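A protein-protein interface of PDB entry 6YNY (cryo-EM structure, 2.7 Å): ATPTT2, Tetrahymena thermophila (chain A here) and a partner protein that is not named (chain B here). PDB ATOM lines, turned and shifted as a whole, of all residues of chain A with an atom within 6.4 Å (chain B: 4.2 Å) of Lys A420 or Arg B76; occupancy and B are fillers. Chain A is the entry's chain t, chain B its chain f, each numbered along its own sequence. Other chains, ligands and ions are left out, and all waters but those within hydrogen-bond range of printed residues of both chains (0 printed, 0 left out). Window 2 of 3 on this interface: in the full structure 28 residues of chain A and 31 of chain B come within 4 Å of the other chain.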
ATOM      1  N   ARG A 418       5.888  -3.176   5.408  1.00  0.00           N
ATOM      2  CA  ARG A 418       5.742  -3.636   4.038  1.00  0.00           C
ATOM      3  C   ARG A 418       6.826  -3.020   3.167  1.00  0.00           C
ATOM      4  O   ARG A 418       7.176  -1.847   3.318  1.00  0.00           O
ATOM      5  CB  ARG A 418       4.367  -3.280   3.484  1.00  0.00           C
ATOM      6  CG  ARG A 418       3.218  -3.576   4.418  1.00  0.00           C
ATOM      7  CD  ARG A 418       1.981  -3.961   3.649  1.00  0.00           C
ATOM      8  NE  ARG A 418       1.720  -3.059   2.535  1.00  0.00           N
ATOM      9  CZ  ARG A 418       0.926  -3.347   1.511  1.00  0.00           C
ATOM     10  NH1 ARG A 418       0.313  -4.518   1.444  1.00  0.00           N
ATOM     11  NH2 ARG A 418       0.754  -2.464   0.547  1.00  0.00           N
ATOM     12  N   ILE A 419       7.353  -3.822   2.245  1.00  0.00           N
ATOM     13  CA  ILE A 419       8.431  -3.363   1.382  1.00  0.00           C
ATOM     14  C   ILE A 419       7.914  -2.302   0.416  1.00  0.00           C
ATOM     15  O   ILE A 419       6.764  -2.346  -0.040  1.00  0.00           O
ATOM     16  CB  ILE A 419       9.050  -4.554   0.628  1.00  0.00           C
ATOM     17  CG1 ILE A 419      10.400  -4.168   0.033  1.00  0.00           C
ATOM     18  CG2 ILE A 419       8.118  -5.034  -0.460  1.00  0.00           C
ATOM     19  CD1 ILE A 419      11.160  -5.336  -0.549  1.00  0.00           C
ATOM     20  N   LYS A 420       8.776  -1.338   0.101  1.00  0.00           N
ATOM     21  CA  LYS A 420       8.436  -0.229  -0.790  1.00  0.00           C
ATOM     22  C   LYS A 420       7.230   0.551  -0.272  1.00  0.00           C
ATOM     23  O   LYS A 420       6.301   0.873  -1.012  1.00  0.00           O
ATOM     24  CB  LYS A 420       8.200  -0.728  -2.216  1.00  0.00           C
ATOM     25  CG  LYS A 420       9.464  -1.239  -2.880  1.00  0.00           C
ATOM     26  CD  LYS A 420       9.295  -1.482  -4.363  1.00  0.00           C
ATOM     27  CE  LYS A 420      10.591  -2.002  -4.969  1.00  0.00           C
ATOM     28  NZ  LYS A 420      10.491  -2.260  -6.432  1.00  0.00           N
ATOM     29  N   SER A 421       7.261   0.863   1.021  1.00  0.00           N
ATOM     30  CA  SER A 421       6.211   1.638   1.662  1.00  0.00           C
ATOM     31  C   SER A 421       6.664   3.028   2.076  1.00  0.00           C
ATOM     32  O   SER A 421       5.831   3.826   2.516  1.00  0.00           O
ATOM     33  CB  SER A 421       5.686   0.902   2.902  1.00  0.00           C
ATOM     34  OG  SER A 421       6.712   0.693   3.850  1.00  0.00           O
ATOM     35  N   ARG A 422       7.949   3.338   1.946  1.00  0.00           N
ATOM     36  CA  ARG A 422       8.494   4.619   2.352  1.00  0.00           C
ATOM     37  C   ARG A 422       9.120   5.319   1.156  1.00  0.00           C
ATOM     38  O   ARG A 422       9.617   4.677   0.227  1.00  0.00           O
ATOM     39  CB  ARG A 422       9.524   4.450   3.466  1.00  0.00           C
ATOM     40  CG  ARG A 422       8.932   3.922   4.758  1.00  0.00           C
ATOM     41  CD  ARG A 422       9.788   4.285   5.941  1.00  0.00           C
ATOM     42  NE  ARG A 422       9.111   4.047   7.211  1.00  0.00           N
ATOM     43  CZ  ARG A 422       9.013   2.861   7.799  1.00  0.00           C
ATOM     44  NH1 ARG A 422       9.541   1.788   7.233  1.00  0.00           N
ATOM     45  NH2 ARG A 422       8.386   2.750   8.954  1.00  0.00           N
ATOM     46  N   TYR A 429      14.621  -1.481   5.221  1.00  0.00           N
ATOM     47  CA  TYR A 429      13.314  -1.847   5.740  1.00  0.00           C
ATOM     48  C   TYR A 429      13.452  -2.779   6.931  1.00  0.00           C
ATOM     49  O   TYR A 429      14.252  -3.718   6.923  1.00  0.00           O
ATOM     50  CB  TYR A 429      12.474  -2.501   4.649  1.00  0.00           C
ATOM     51  CG  TYR A 429      11.825  -1.498   3.734  1.00  0.00           C
ATOM     52  CD1 TYR A 429      10.592  -0.956   4.041  1.00  0.00           C
ATOM     53  CD2 TYR A 429      12.450  -1.083   2.573  1.00  0.00           C
ATOM     54  CE1 TYR A 429       9.995  -0.038   3.219  1.00  0.00           C
ATOM     55  CE2 TYR A 429      11.860  -0.160   1.742  1.00  0.00           C
ATOM     56  CZ  TYR A 429      10.631   0.360   2.072  1.00  0.00           C
ATOM     57  OH  TYR A 429      10.035   1.280   1.248  1.00  0.00           O
ATOM     58  N   ARG B  27       0.000   2.585  -0.152  1.00  0.00           N
ATOM     59  CA  ARG B  27      -0.107   3.218  -1.455  1.00  0.00           C
ATOM     60  C   ARG B  27      -1.204   2.597  -2.307  1.00  0.00           C
ATOM     61  O   ARG B  27      -1.140   2.666  -3.538  1.00  0.00           O
ATOM     62  CB  ARG B  27       1.237   3.152  -2.174  1.00  0.00           C
ATOM     63  CG  ARG B  27       2.387   3.684  -1.340  1.00  0.00           C
ATOM     64  CD  ARG B  27       3.667   3.799  -2.141  1.00  0.00           C
ATOM     65  NE  ARG B  27       4.779   4.261  -1.319  1.00  0.00           N
ATOM     66  CZ  ARG B  27       4.966   5.524  -0.954  1.00  0.00           C
ATOM     67  NH1 ARG B  27       6.009   5.845  -0.206  1.00  0.00           N
ATOM     68  NH2 ARG B  27       4.112   6.467  -1.330  1.00  0.00           N
ATOM     69  N   ASN B  74       2.946  -6.029  -1.791  1.00  0.00           N
ATOM     70  CA  ASN B  74       2.806  -7.471  -1.912  1.00  0.00           C
ATOM     71  C   ASN B  74       3.864  -8.092  -2.807  1.00  0.00           C
ATOM     72  O   ASN B  74       3.799  -9.294  -3.078  1.00  0.00           O
ATOM     73  CB  ASN B  74       1.419  -7.822  -2.449  1.00  0.00           C
ATOM     74  CG  ASN B  74       0.451  -8.206  -1.360  1.00  0.00           C
ATOM     75  OD1 ASN B  74       0.440  -9.344  -0.898  1.00  0.00           O
ATOM     76  ND2 ASN B  74      -0.379  -7.264  -0.951  1.00  0.00           N
ATOM     77  N   LYS B  75       4.826  -7.307  -3.276  1.00  0.00           N
ATOM     78  CA  LYS B  75       5.855  -7.843  -4.149  1.00  0.00           C
ATOM     79  C   LYS B  75       6.677  -8.902  -3.429  1.00  0.00           C
ATOM     80  O   LYS B  75       7.019  -8.760  -2.254  1.00  0.00           O
ATOM     81  CB  LYS B  75       6.772  -6.727  -4.643  1.00  0.00           C
ATOM     82  CG  LYS B  75       6.238  -5.945  -5.815  1.00  0.00           C
ATOM     83  CD  LYS B  75       7.265  -4.959  -6.317  1.00  0.00           C
ATOM     84  CE  LYS B  75       6.745  -4.120  -7.459  1.00  0.00           C
ATOM     85  NZ  LYS B  75       6.520  -4.922  -8.683  1.00  0.00           N
ATOM     86  N   ARG B  76       6.986  -9.977  -4.153  1.00  0.00           N
ATOM     87  CA  ARG B  76       7.891 -11.020  -3.683  1.00  0.00           C
ATOM     88  C   ARG B  76       7.399 -11.665  -2.393  1.00  0.00           C
ATOM     89  O   ARG B  76       8.191 -12.163  -1.594  1.00  0.00           O
ATOM     90  CB  ARG B  76       9.303 -10.463  -3.506  1.00  0.00           C
ATOM     91  CG  ARG B  76       9.948 -10.066  -4.813  1.00  0.00           C
ATOM     92  CD  ARG B  76      11.303  -9.429  -4.620  1.00  0.00           C
ATOM     93  NE  ARG B  76      11.215  -8.096  -4.035  1.00  0.00           N
ATOM     94  CZ  ARG B  76      11.021  -6.980  -4.729  1.00  0.00           C
ATOM     95  NH1 ARG B  76      10.884  -7.017  -6.043  1.00  0.00           N
ATOM     96  NH2 ARG B  76      10.956  -5.817  -4.104  1.00  0.00           N
ATOM     97  N   ARG B  77       6.084 -11.686  -2.198  1.00  0.00           N
ATOM     98  CA  ARG B  77       5.514 -12.233  -0.975  1.00  0.00           C
ATOM     99  C   ARG B  77       5.552 -13.753  -0.960  1.00  0.00           C
ATOM    100  O   ARG B  77       5.671 -14.355   0.111  1.00  0.00           O
ATOM    101  CB  ARG B  77       4.081 -11.740  -0.814  1.00  0.00           C
ATOM    102  CG  ARG B  77       3.451 -12.069   0.502  1.00  0.00           C
ATOM    103  CD  ARG B  77       2.108 -11.426   0.604  1.00  0.00           C
ATOM    104  NE  ARG B  77       1.457 -11.703   1.872  1.00  0.00           N
ATOM    105  CZ  ARG B  77       0.254 -11.252   2.204  1.00  0.00           C
ATOM    106  NH1 ARG B  77      -0.432 -10.502   1.361  1.00  0.00           N
ATOM    107  NH2 ARG B  77      -0.264 -11.552   3.380  1.00  0.00           N
ATOM    108  N   TRP B  78       5.449 -14.384  -2.127  1.00  0.00           N
ATOM    109  CA  TRP B  78       5.520 -15.837  -2.191  1.00  0.00           C
ATOM    110  C   TRP B  78       6.926 -16.330  -1.879  1.00  0.00           C
ATOM    111  O   TRP B  78       7.097 -17.306  -1.140  1.00  0.00           O
ATOM    112  CB  TRP B  78       5.072 -16.307  -3.567  1.00  0.00           C
ATOM    113  CG  TRP B  78       5.038 -17.775  -3.731  1.00  0.00           C
ATOM    114  CD1 TRP B  78       4.021 -18.608  -3.394  1.00  0.00           C
ATOM    115  CD2 TRP B  78       6.064 -18.598  -4.288  1.00  0.00           C
ATOM    116  NE1 TRP B  78       4.348 -19.901  -3.702  1.00  0.00           N
ATOM    117  CE2 TRP B  78       5.601 -19.922  -4.251  1.00  0.00           C
ATOM    118  CE3 TRP B  78       7.332 -18.344  -4.811  1.00  0.00           C
ATOM    119  CZ2 TRP B  78       6.358 -20.986  -4.713  1.00  0.00           C
ATOM    120  CZ3 TRP B  78       8.079 -19.400  -5.270  1.00  0.00           C
ATOM    121  CH2 TRP B  78       7.592 -20.705  -5.220  1.00  0.00           C
ATOM    122  N   PHE B  79       7.944 -15.672  -2.434  1.00  0.00           N
ATOM    123  CA  PHE B  79       9.320 -16.027  -2.109  1.00  0.00           C
ATOM    124  C   PHE B  79       9.591 -15.881  -0.618  1.00  0.00           C
ATOM    125  O   PHE B  79      10.262 -16.724  -0.015  1.00  0.00           O
ATOM    126  CB  PHE B  79      10.292 -15.153  -2.898  1.00  0.00           C
ATOM    127  CG  PHE B  79      10.428 -15.531  -4.336  1.00  0.00           C
ATOM    128  CD1 PHE B  79      11.083 -16.689  -4.701  1.00  0.00           C
ATOM    129  CD2 PHE B  79       9.925 -14.714  -5.327  1.00  0.00           C
ATOM    130  CE1 PHE B  79      11.217 -17.031  -6.021  1.00  0.00           C
ATOM    131  CE2 PHE B  79      10.057 -15.053  -6.647  1.00  0.00           C
ATOM    132  CZ  PHE B  79      10.705 -16.211  -6.997  1.00  0.00           C
ATOM    133  N   LYS B  80       9.077 -14.814  -0.008  1.00  0.00           N
ATOM    134  CA  LYS B  80       9.374 -14.538   1.392  1.00  0.00           C
ATOM    135  C   LYS B  80       8.766 -15.579   2.320  1.00  0.00           C
ATOM    136  O   LYS B  80       9.408 -16.002   3.288  1.00  0.00           O
ATOM    137  CB  LYS B  80       8.884 -13.140   1.750  1.00  0.00           C
ATOM    138  CG  LYS B  80       9.702 -12.053   1.111  1.00  0.00           C
ATOM    139  CD  LYS B  80       9.113 -10.694   1.353  1.00  0.00           C
ATOM    140  CE  LYS B  80      10.004  -9.623   0.787  1.00  0.00           C
ATOM    141  NZ  LYS B  80       9.528  -8.278   1.143  1.00  0.00           N
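NH1 of Arg B27 lies within hydrogen-bond range of O of Ser A421 (3.4 Å).
The side-chain hydroxyl of Ser A421 lies within hydrogen-bond range of the backbone carbonyl oxygen of Arg A418 (2.6 Å). The backbone NH (N) of Lys A420 sits close to the side-chain hydroxyl (OH) of Tyr A429 (3.1 Å). The backbone NH (N) of Ser A421 lies within hydrogen-bond range of the side-chain hydroxyl (OH) of Tyr A429, at 2.8 Å. N of Arg A422 lies within hydrogen-bond range of OH of Tyr A429. NH1 of Arg B77 lies within hydrogen-bond range of OD1 of Asn B74, 2.7 Å away.
ND2 of Asn B74 touches NH1 of Arg A418 (3.7 Å). Arg B76 touches Ile A419. Lys B80 touches Ile A419 (NZ to CD1, 3.8 Å). Lys A420 touches Arg B27. Lys A420 touches Arg B76 (CE to NH2, 3.9 Å). Arg B27 touches Arg A422 (NH1 to C, 3.4 Å).
Of the printed residues of chain A, Arg B76 touches Ile A419 (3.6 Å) and Lys A420 (3.9 Å). Printed residues of chain B within 4 Å of Arg A418: Asn B74. Of the printed residues of chain B, Ser A421 touches Arg B27 (3.4 Å). Printed residues of chain B within 4 Å of Arg A422: Arg B27 (3.4 Å). Of the printed residues of chain A, Arg B27 touches Lys A420 (3.7 Å), Ser A421 (3.4 Å) and Arg A422 (3.4 Å). The nearest printed residue of chain A that does not touch Arg B76 is Tyr A429 (8.2 Å).
Of the 8 printed residues of chain B, 4 touch a printed residue of chain A. Printed residues of chain B that touch a printed residue of chain A: Arg B27, Asn B74, Arg B76 and Lys B80. Of the 6 printed residues of chain A, 5 touch a printed residue of chain B. Hydrophobic or aromatic side chains of chain A that line the printed part of chain B: Ile A419. Among the printed residues, 7 pairs touch across the chains. Among the printed residues, no Asp or Glu carboxylate lies within 4 Å of a Lys or Arg side-chain nitrogen of the other chain.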
